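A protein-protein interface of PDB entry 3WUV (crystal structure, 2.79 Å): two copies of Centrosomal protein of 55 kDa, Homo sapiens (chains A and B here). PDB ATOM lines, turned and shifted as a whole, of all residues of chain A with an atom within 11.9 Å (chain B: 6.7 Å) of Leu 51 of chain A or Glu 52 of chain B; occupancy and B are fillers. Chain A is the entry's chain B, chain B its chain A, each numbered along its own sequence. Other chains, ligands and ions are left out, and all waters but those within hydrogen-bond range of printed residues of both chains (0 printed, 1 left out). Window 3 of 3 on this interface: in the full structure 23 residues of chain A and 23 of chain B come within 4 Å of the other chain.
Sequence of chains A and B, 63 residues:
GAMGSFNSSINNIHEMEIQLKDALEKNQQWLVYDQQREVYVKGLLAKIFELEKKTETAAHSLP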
ATOM      1  N   TYR A  40      12.046  15.405 -17.045  1.00  0.00           N
ATOM      2  CA  TYR A  40      10.896  14.774 -16.409  1.00  0.00           C
ATOM      3  C   TYR A  40       9.903  14.251 -17.440  1.00  0.00           C
ATOM      4  O   TYR A  40       9.473  13.099 -17.373  1.00  0.00           O
ATOM      5  CB  TYR A  40      10.199  15.750 -15.460  1.00  0.00           C
ATOM      6  CG  TYR A  40       9.108  15.103 -14.641  1.00  0.00           C
ATOM      7  CD1 TYR A  40       9.406  14.090 -13.739  1.00  0.00           C
ATOM      8  CD2 TYR A  40       7.783  15.498 -14.768  1.00  0.00           C
ATOM      9  CE1 TYR A  40       8.416  13.486 -12.988  1.00  0.00           C
ATOM     10  CE2 TYR A  40       6.782  14.898 -14.015  1.00  0.00           C
ATOM     11  CZ  TYR A  40       7.107  13.892 -13.128  1.00  0.00           C
ATOM     12  OH  TYR A  40       6.126  13.288 -12.375  1.00  0.00           O
ATOM     13  N   LYS A  42      10.392  13.536 -20.565  1.00  0.00           N
ATOM     14  CA  LYS A  42      10.995  12.449 -21.337  1.00  0.00           C
ATOM     15  C   LYS A  42      10.974  11.131 -20.580  1.00  0.00           C
ATOM     16  O   LYS A  42      10.795  10.066 -21.173  1.00  0.00           O
ATOM     17  CB  LYS A  42      12.434  12.791 -21.717  1.00  0.00           C
ATOM     18  CG  LYS A  42      12.568  13.915 -22.722  1.00  0.00           C
ATOM     19  CD  LYS A  42      14.029  14.183 -23.029  1.00  0.00           C
ATOM     20  CE  LYS A  42      14.191  15.283 -24.064  1.00  0.00           C
ATOM     21  NZ  LYS A  42      15.624  15.635 -24.278  1.00  0.00           N
ATOM     22  N   GLY A  43      11.174  11.207 -19.269  1.00  0.00           N
ATOM     23  CA  GLY A  43      11.113  10.030 -18.425  1.00  0.00           C
ATOM     24  C   GLY A  43       9.704   9.477 -18.363  1.00  0.00           C
ATOM     25  O   GLY A  43       9.499   8.263 -18.358  1.00  0.00           O
ATOM     26  N   LEU A  44       8.729  10.380 -18.311  1.00  0.00           N
ATOM     27  CA  LEU A  44       7.321  10.006 -18.339  1.00  0.00           C
ATOM     28  C   LEU A  44       6.976   9.359 -19.679  1.00  0.00           C
ATOM     29  O   LEU A  44       6.256   8.361 -19.734  1.00  0.00           O
ATOM     30  CB  LEU A  44       6.453  11.245 -18.106  1.00  0.00           C
ATOM     31  CG  LEU A  44       5.676  11.347 -16.791  1.00  0.00           C
ATOM     32  CD1 LEU A  44       6.488  10.794 -15.644  1.00  0.00           C
ATOM     33  CD2 LEU A  44       5.282  12.790 -16.516  1.00  0.00           C
ATOM     34  N   LEU A  45       7.496   9.941 -20.755  1.00  0.00           N
ATOM     35  CA  LEU A  45       7.325   9.387 -22.094  1.00  0.00           C
ATOM     36  C   LEU A  45       7.936   7.993 -22.175  1.00  0.00           C
ATOM     37  O   LEU A  45       7.354   7.081 -22.765  1.00  0.00           O
ATOM     38  CB  LEU A  45       7.975  10.300 -23.137  1.00  0.00           C
ATOM     39  CG  LEU A  45       7.080  11.216 -23.975  1.00  0.00           C
ATOM     40  CD1 LEU A  45       5.684  11.314 -23.394  1.00  0.00           C
ATOM     41  CD2 LEU A  45       7.705  12.595 -24.092  1.00  0.00           C
ATOM     42  N   ALA A  46       9.113   7.841 -21.578  1.00  0.00           N
ATOM     43  CA  ALA A  46       9.808   6.560 -21.559  1.00  0.00           C
ATOM     44  C   ALA A  46       9.005   5.510 -20.801  1.00  0.00           C
ATOM     45  O   ALA A  46       8.925   4.357 -21.221  1.00  0.00           O
ATOM     46  CB  ALA A  46      11.190   6.716 -20.951  1.00  0.00           C
ATOM     47  N   LYS A  47       8.413   5.919 -19.683  1.00  0.00           N
ATOM     48  CA  LYS A  47       7.551   5.040 -18.902  1.00  0.00           C
ATOM     49  C   LYS A  47       6.402   4.514 -19.760  1.00  0.00           C
ATOM     50  O   LYS A  47       6.161   3.310 -19.806  1.00  0.00           O
ATOM     51  CB  LYS A  47       7.011   5.783 -17.679  1.00  0.00           C
ATOM     52  CG  LYS A  47       6.141   4.945 -16.765  1.00  0.00           C
ATOM     53  CD  LYS A  47       6.909   3.771 -16.191  1.00  0.00           C
ATOM     54  CE  LYS A  47       6.064   3.015 -15.183  1.00  0.00           C
ATOM     55  NZ  LYS A  47       6.709   1.742 -14.768  1.00  0.00           N
ATOM     56  N   ILE A  48       5.714   5.426 -20.442  1.00  0.00           N
ATOM     57  CA  ILE A  48       4.624   5.087 -21.357  1.00  0.00           C
ATOM     58  C   ILE A  48       5.066   4.108 -22.443  1.00  0.00           C
ATOM     59  O   ILE A  48       4.449   3.060 -22.636  1.00  0.00           O
ATOM     60  CB  ILE A  48       4.063   6.353 -22.036  1.00  0.00           C
ATOM     61  CG1 ILE A  48       3.350   7.234 -21.011  1.00  0.00           C
ATOM     62  CG2 ILE A  48       3.125   5.984 -23.177  1.00  0.00           C
ATOM     63  CD1 ILE A  48       2.923   8.583 -21.549  1.00  0.00           C
ATOM     64  N   PHE A  49       6.133   4.476 -23.148  1.00  0.00           N
ATOM     65  CA  PHE A  49       6.740   3.641 -24.182  1.00  0.00           C
ATOM     66  C   PHE A  49       6.941   2.217 -23.680  1.00  0.00           C
ATOM     67  O   PHE A  49       6.463   1.256 -24.286  1.00  0.00           O
ATOM     68  CB  PHE A  49       8.089   4.241 -24.589  1.00  0.00           C
ATOM     69  CG  PHE A  49       8.812   3.470 -25.658  1.00  0.00           C
ATOM     70  CD1 PHE A  49       9.548   2.336 -25.347  1.00  0.00           C
ATOM     71  CD2 PHE A  49       8.785   3.900 -26.972  1.00  0.00           C
ATOM     72  CE1 PHE A  49      10.216   1.631 -26.328  1.00  0.00           C
ATOM     73  CE2 PHE A  49       9.459   3.202 -27.957  1.00  0.00           C
ATOM     74  CZ  PHE A  49      10.173   2.067 -27.635  1.00  0.00           C
ATOM     75  N   GLU A  50       7.668   2.097 -22.576  1.00  0.00           N
ATOM     76  CA  GLU A  50       7.911   0.815 -21.935  1.00  0.00           C
ATOM     77  C   GLU A  50       6.604   0.153 -21.521  1.00  0.00           C
ATOM     78  O   GLU A  50       6.404  -1.041 -21.734  1.00  0.00           O
ATOM     79  CB  GLU A  50       8.797   1.020 -20.706  1.00  0.00           C
ATOM     80  CG  GLU A  50       8.594  -0.004 -19.606  1.00  0.00           C
ATOM     81  CD  GLU A  50       9.009   0.521 -18.246  1.00  0.00           C
ATOM     82  OE1 GLU A  50      10.108   1.107 -18.146  1.00  0.00           O
ATOM     83  OE2 GLU A  50       8.228   0.364 -17.282  1.00  0.00           O
ATOM     84  N   LEU A  51       5.711   0.941 -20.933  1.00  0.00           N
ATOM     85  CA  LEU A  51       4.458   0.413 -20.417  1.00  0.00           C
ATOM     86  C   LEU A  51       3.552  -0.081 -21.536  1.00  0.00           C
ATOM     87  O   LEU A  51       2.718  -0.961 -21.324  1.00  0.00           O
ATOM     88  CB  LEU A  51       3.734   1.484 -19.604  1.00  0.00           C
ATOM     89  CG  LEU A  51       3.089   1.032 -18.300  1.00  0.00           C
ATOM     90  CD1 LEU A  51       3.973   0.018 -17.609  1.00  0.00           C
ATOM     91  CD2 LEU A  51       2.863   2.236 -17.408  1.00  0.00           C
ATOM     92  N   GLU A  52       3.716   0.484 -22.727  1.00  0.00           N
ATOM     93  CA  GLU A  52       2.818   0.168 -23.829  1.00  0.00           C
ATOM     94  C   GLU A  52       2.934  -1.297 -24.225  1.00  0.00           C
ATOM     95  O   GLU A  52       3.638  -1.657 -25.180  1.00  0.00           O
ATOM     96  CB  GLU A  52       3.033   1.114 -25.011  1.00  0.00           C
ATOM     97  CG  GLU A  52       1.866   2.085 -25.167  1.00  0.00           C
ATOM     98  CD  GLU A  52       2.255   3.367 -25.859  1.00  0.00           C
ATOM     99  OE1 GLU A  52       1.470   4.334 -25.777  1.00  0.00           O
ATOM    100  OE2 GLU A  52       3.337   3.411 -26.484  1.00  0.00           O
ATOM    101  N   LYS A  53       2.234  -2.137 -23.468  1.00  0.00           N
ATOM    102  CA  LYS A  53       2.353  -3.575 -23.638  1.00  0.00           C
ATOM    103  C   LYS A  53       1.191  -4.167 -24.418  1.00  0.00           C
ATOM    104  O   LYS A  53       0.098  -4.388 -23.887  1.00  0.00           O
ATOM    105  CB  LYS A  53       2.585  -4.285 -22.300  1.00  0.00           C
ATOM    106  CG  LYS A  53       4.066  -4.540 -22.020  1.00  0.00           C
ATOM    107  CD  LYS A  53       4.845  -4.702 -23.330  1.00  0.00           C
ATOM    108  CE  LYS A  53       5.863  -3.579 -23.517  1.00  0.00           C
ATOM    109  NZ  LYS A  53       5.760  -2.858 -24.819  1.00  0.00           N
ATOM    110  N   LYS A  54       1.458  -4.382 -25.703  1.00  0.00           N
ATOM    111  CA  LYS A  54       0.499  -4.923 -26.654  1.00  0.00           C
ATOM    112  C   LYS A  54      -0.696  -3.996 -26.876  1.00  0.00           C
ATOM    113  O   LYS A  54      -1.704  -4.399 -27.456  1.00  0.00           O
ATOM    114  CB  LYS A  54       0.071  -6.335 -26.247  1.00  0.00           C
ATOM    115  CG  LYS A  54       1.257  -7.248 -25.964  1.00  0.00           C
ATOM    116  CD  LYS A  54       0.837  -8.681 -25.694  1.00  0.00           C
ATOM    117  CE  LYS A  54       1.538  -9.630 -26.652  1.00  0.00           C
ATOM    118  NZ  LYS A  54       2.979  -9.284 -26.813  1.00  0.00           N
ATOM    119  N   THR A  55      -0.573  -2.749 -26.428  1.00  0.00           N
ATOM    120  CA  THR A  55      -1.602  -1.749 -26.684  1.00  0.00           C
ATOM    121  C   THR A  55      -1.107  -0.732 -27.706  1.00  0.00           C
ATOM    122  O   THR A  55      -1.904  -0.057 -28.350  1.00  0.00           O
ATOM    123  CB  THR A  55      -2.065  -1.032 -25.401  1.00  0.00           C
ATOM    124  OG1 THR A  55      -1.023  -0.176 -24.919  1.00  0.00           O
ATOM    125  CG2 THR A  55      -2.434  -2.050 -24.330  1.00  0.00           C
ATOM    126  N   GLU A  56       0.211  -0.627 -27.841  1.00  0.00           N
ATOM    127  CA  GLU A  56       0.817   0.090 -28.961  1.00  0.00           C
ATOM    128  C   GLU A  56       2.215  -0.424 -29.293  1.00  0.00           C
ATOM    129  O   GLU A  56       2.779  -1.253 -28.578  1.00  0.00           O
ATOM    130  CB  GLU A  56       0.841   1.612 -28.749  1.00  0.00           C
ATOM    131  CG  GLU A  56      -0.410   2.365 -29.244  1.00  0.00           C
ATOM    132  CD  GLU A  56      -0.813   2.032 -30.685  1.00  0.00           C
ATOM    133  OE1 GLU A  56       0.050   1.597 -31.480  1.00  0.00           O
ATOM    134  OE2 GLU A  56      -2.004   2.208 -31.026  1.00  0.00           O
ATOM    135  N   THR A  57       2.764   0.093 -30.384  1.00  0.00           N
ATOM    136  CA  THR A  57       3.996  -0.419 -30.960  1.00  0.00           C
ATOM    137  C   THR A  57       4.791   0.720 -31.578  1.00  0.00           C
ATOM    138  O   THR A  57       4.240   1.559 -32.289  1.00  0.00           O
ATOM    139  CB  THR A  57       3.670  -1.429 -32.054  1.00  0.00           C
ATOM    140  OG1 THR A  57       4.679  -1.385 -33.071  1.00  0.00           O
ATOM    141  CG2 THR A  57       2.345  -1.068 -32.668  1.00  0.00           C
ATOM    142  N   ALA A  58       6.090   0.752 -31.298  1.00  0.00           N
ATOM    143  CA  ALA A  58       6.955   1.799 -31.822  1.00  0.00           C
ATOM    144  C   ALA A  58       8.107   1.192 -32.610  1.00  0.00           C
ATOM    145  O   ALA A  58       8.098  -0.004 -32.910  1.00  0.00           O
ATOM    146  CB  ALA A  58       7.475   2.674 -30.691  1.00  0.00           C
ATOM    147  N   LYS B  47      -2.425   8.936 -18.466  1.00  0.00           N
ATOM    148  CA  LYS B  47      -2.188   7.880 -19.437  1.00  0.00           C
ATOM    149  C   LYS B  47      -1.468   6.700 -18.797  1.00  0.00           C
ATOM    150  O   LYS B  47      -1.855   5.548 -18.989  1.00  0.00           O
ATOM    151  CB  LYS B  47      -1.371   8.425 -20.608  1.00  0.00           C
ATOM    152  CG  LYS B  47      -1.286   7.486 -21.798  1.00  0.00           C
ATOM    153  CD  LYS B  47      -0.737   8.197 -23.022  1.00  0.00           C
ATOM    154  CE  LYS B  47      -0.902   7.344 -24.265  1.00  0.00           C
ATOM    155  NZ  LYS B  47      -0.480   8.059 -25.500  1.00  0.00           N
ATOM    156  N   ILE B  48      -0.421   7.001 -18.034  1.00  0.00           N
ATOM    157  CA  ILE B  48       0.358   5.982 -17.340  1.00  0.00           C
ATOM    158  C   ILE B  48      -0.508   5.191 -16.363  1.00  0.00           C
ATOM    159  O   ILE B  48      -0.417   3.966 -16.291  1.00  0.00           O
ATOM    160  CB  ILE B  48       1.549   6.609 -16.584  1.00  0.00           C
ATOM    161  CG1 ILE B  48       2.555   7.201 -17.572  1.00  0.00           C
ATOM    162  CG2 ILE B  48       2.232   5.578 -15.703  1.00  0.00           C
ATOM    163  CD1 ILE B  48       3.758   7.840 -16.913  1.00  0.00           C
ATOM    164  N   PHE B  49      -1.352   5.901 -15.619  1.00  0.00           N
ATOM    165  CA  PHE B  49      -2.270   5.271 -14.677  1.00  0.00           C
ATOM    166  C   PHE B  49      -3.151   4.241 -15.377  1.00  0.00           C
ATOM    167  O   PHE B  49      -3.262   3.100 -14.928  1.00  0.00           O
ATOM    168  CB  PHE B  49      -3.141   6.327 -13.994  1.00  0.00           C
ATOM    169  CG  PHE B  49      -4.093   5.764 -12.981  1.00  0.00           C
ATOM    170  CD1 PHE B  49      -3.657   5.439 -11.709  1.00  0.00           C
ATOM    171  CD2 PHE B  49      -5.427   5.562 -13.299  1.00  0.00           C
ATOM    172  CE1 PHE B  49      -4.530   4.922 -10.772  1.00  0.00           C
ATOM    173  CE2 PHE B  49      -6.306   5.044 -12.365  1.00  0.00           C
ATOM    174  CZ  PHE B  49      -5.855   4.724 -11.100  1.00  0.00           C
ATOM    175  N   GLU B  50      -3.767   4.652 -16.480  1.00  0.00           N
ATOM    176  CA  GLU B  50      -4.631   3.776 -17.260  1.00  0.00           C
ATOM    177  C   GLU B  50      -3.860   2.579 -17.807  1.00  0.00           C
ATOM    178  O   GLU B  50      -4.296   1.433 -17.692  1.00  0.00           O
ATOM    179  CB  GLU B  50      -5.262   4.558 -18.412  1.00  0.00           C
ATOM    180  CG  GLU B  50      -6.762   4.417 -18.477  1.00  0.00           C
ATOM    181  CD  GLU B  50      -7.406   4.643 -17.130  1.00  0.00           C
ATOM    182  OE1 GLU B  50      -8.084   3.719 -16.635  1.00  0.00           O
ATOM    183  OE2 GLU B  50      -7.228   5.742 -16.564  1.00  0.00           O
ATOM    184  N   LEU B  51      -2.707   2.868 -18.402  1.00  0.00           N
ATOM    185  CA  LEU B  51      -1.820   1.857 -18.963  1.00  0.00           C
ATOM    186  C   LEU B  51      -1.410   0.831 -17.907  1.00  0.00           C
ATOM    187  O   LEU B  51      -1.190  -0.341 -18.216  1.00  0.00           O
ATOM    188  CB  LEU B  51      -0.577   2.547 -19.531  1.00  0.00           C
ATOM    189  CG  LEU B  51      -0.099   2.240 -20.949  1.00  0.00           C
ATOM    190  CD1 LEU B  51      -1.230   1.704 -21.801  1.00  0.00           C
ATOM    191  CD2 LEU B  51       0.497   3.491 -21.582  1.00  0.00           C
ATOM    192  N   GLU B  52      -1.314   1.279 -16.659  1.00  0.00           N
ATOM    193  CA  GLU B  52      -0.878   0.418 -15.564  1.00  0.00           C
ATOM    194  C   GLU B  52      -1.993  -0.469 -15.018  1.00  0.00           C
ATOM    195  O   GLU B  52      -1.756  -1.316 -14.157  1.00  0.00           O
ATOM    196  CB  GLU B  52      -0.262   1.254 -14.438  1.00  0.00           C
ATOM    197  CG  GLU B  52       1.252   1.169 -14.378  1.00  0.00           C
ATOM    198  CD  GLU B  52       1.875   2.285 -13.561  1.00  0.00           C
ATOM    199  OE1 GLU B  52       1.128   3.025 -12.884  1.00  0.00           O
ATOM    200  OE2 GLU B  52       3.116   2.425 -13.603  1.00  0.00           O
ATOM    201  N   LYS B  53      -3.210  -0.275 -15.515  1.00  0.00           N
ATOM    202  CA  LYS B  53      -4.324  -1.119 -15.106  1.00  0.00           C
ATOM    203  C   LYS B  53      -4.338  -2.387 -15.945  1.00  0.00           C
ATOM    204  O   LYS B  53      -4.914  -3.401 -15.554  1.00  0.00           O
ATOM    205  CB  LYS B  53      -5.652  -0.381 -15.252  1.00  0.00           C
ATOM    206  CG  LYS B  53      -5.808   0.822 -14.342  1.00  0.00           C
ATOM    207  CD  LYS B  53      -7.201   1.411 -14.475  1.00  0.00           C
ATOM    208  CE  LYS B  53      -8.260   0.420 -14.022  1.00  0.00           C
ATOM    209  NZ  LYS B  53      -8.199   0.185 -12.553  1.00  0.00           N
ATOM    210  N   LYS B  54      -3.693  -2.323 -17.103  1.00  0.00           N
ATOM    211  CA  LYS B  54      -3.614  -3.469 -17.993  1.00  0.00           C
ATOM    212  C   LYS B  54      -2.429  -4.338 -17.603  1.00  0.00           C
ATOM    213  O   LYS B  54      -2.315  -5.486 -18.032  1.00  0.00           O
ATOM    214  CB  LYS B  54      -3.492  -2.996 -19.437  1.00  0.00           C
ATOM    215  CG  LYS B  54      -4.393  -1.811 -19.732  1.00  0.00           C
ATOM    216  CD  LYS B  54      -4.535  -1.561 -21.217  1.00  0.00           C
ATOM    217  CE  LYS B  54      -6.000  -1.546 -21.621  1.00  0.00           C
ATOM    218  NZ  LYS B  54      -6.630  -2.888 -21.472  1.00  0.00           N
ATOM    219  N   THR B  55      -1.550  -3.779 -16.777  1.00  0.00           N
ATOM    220  CA  THR B  55      -0.426  -4.527 -16.236  1.00  0.00           C
ATOM    221  C   THR B  55      -0.907  -5.369 -15.059  1.00  0.00           C
ATOM    222  O   THR B  55      -0.281  -6.365 -14.694  1.00  0.00           O
ATOM    223  CB  THR B  55       0.727  -3.591 -15.793  1.00  0.00           C
ATOM    224  OG1 THR B  55       1.985  -4.182 -16.135  1.00  0.00           O
ATOM    225  CG2 THR B  55       0.683  -3.323 -14.288  1.00  0.00           C
ATOM    226  N   GLU B  56      -2.034  -4.964 -14.480  1.00  0.00           N
ATOM    227  CA  GLU B  56      -2.609  -5.654 -13.332  1.00  0.00           C
ATOM    228  C   GLU B  56      -3.106  -7.042 -13.710  1.00  0.00           C
ATOM    229  O   GLU B  56      -4.280  -7.225 -14.022  1.00  0.00           O
ATOM    230  CB  GLU B  56      -3.752  -4.831 -12.735  1.00  0.00           C
ATOM    231  CG  GLU B  56      -3.289  -3.606 -11.966  1.00  0.00           C
ATOM    232  CD  GLU B  56      -4.441  -2.739 -11.495  1.00  0.00           C
ATOM    233  OE1 GLU B  56      -5.608  -3.078 -11.794  1.00  0.00           O
ATOM    234  OE2 GLU B  56      -4.179  -1.716 -10.828  1.00  0.00           O
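OE2 of Glu 52 of chain B lies within salt-bridge range of NZ of Lys 47 of chain A, 3.8 Å away.
OE2 of Glu 50 of chain A lies within salt-bridge range of NZ of Lys 47 of chain A, at 3.2 Å.
Among the printed residues, merely in contact across the chains: Leu 44 of chain A with Ile 48 of chain B, Lys 47 of chain A with Ile 48 of chain B, Ile 48 of chain A with Lys 47 of chain B, Ile 48 of chain A with Ile 48 of chain B, Ile 48 of chain A with Leu 51 of chain B, Leu 51 of chain A with Ile 48 of chain B, Leu 51 of chain A with Glu 52 of chain B, Thr 55 of chain A with Leu 51 of chain B and Thr 55 of chain A with Lys 54 of chain B.
Of the printed residues of chain B, Ile 48 of chain A touches Lys 47 (3.96 Å), Ile 48 (3.5 Å) and Leu 51 (3.96 Å).
Of chain B, only Ile 48 and Glu 52 come within 4 Å of Leu 51 of chain A.
Of the printed residues of chain A, Lys 47 of chain B touches Ile 48.
Of chain A, only Ile 48 (3.96 Å) and Thr 55 (3.6 Å) come within 4 Å of Leu 51 of chain B.
Printed residues of chain A within 4 Å of Glu 52 of chain B: Lys 47 (3.4 Å) and Leu 51 (3.6 Å).
Of the printed residues of chain A, Lys 54 of chain B touches Thr 55.
Thr 55 of chain B touches none of the printed residues of chain A.
The nearest printed residue of chain B that does not touch Lys 47 of chain A is Leu 51 of chain B (5.9 Å).
Of the 18 printed residues of chain A, 5 touch a printed residue of chain B.
Hydrophobic or aromatic side chains of chain B that line the printed part of chain A: Ile 48 and Leu 51.
Among the printed residues, 10 pairs touch across the chains.
Among the printed residues, Asp or Glu carboxylates within 4 Å of a Lys or Arg side-chain nitrogen of the other chain: Lys 47 of chain A with Glu 52 of chain B (3.8 Å).
Ile 48 of chain A touches its own counterpart, Ile 48 of chain B.
Leu 51 of chain A touches Glu 52 of chain B, but with the chains exchanged Glu 52 of chain A does not touch Leu 51 of chain B (4.1 Å).
Thr 55 of chain A touches Leu 51 of chain B, but with the chains exchanged Leu 51 of chain A does not touch Thr 55 of chain B (4.9 Å).
Thr 55 of chain A touches Lys 54 of chain B, but with the chains exchanged Lys 54 of chain A does not touch Thr 55 of chain B (9.4 Å).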
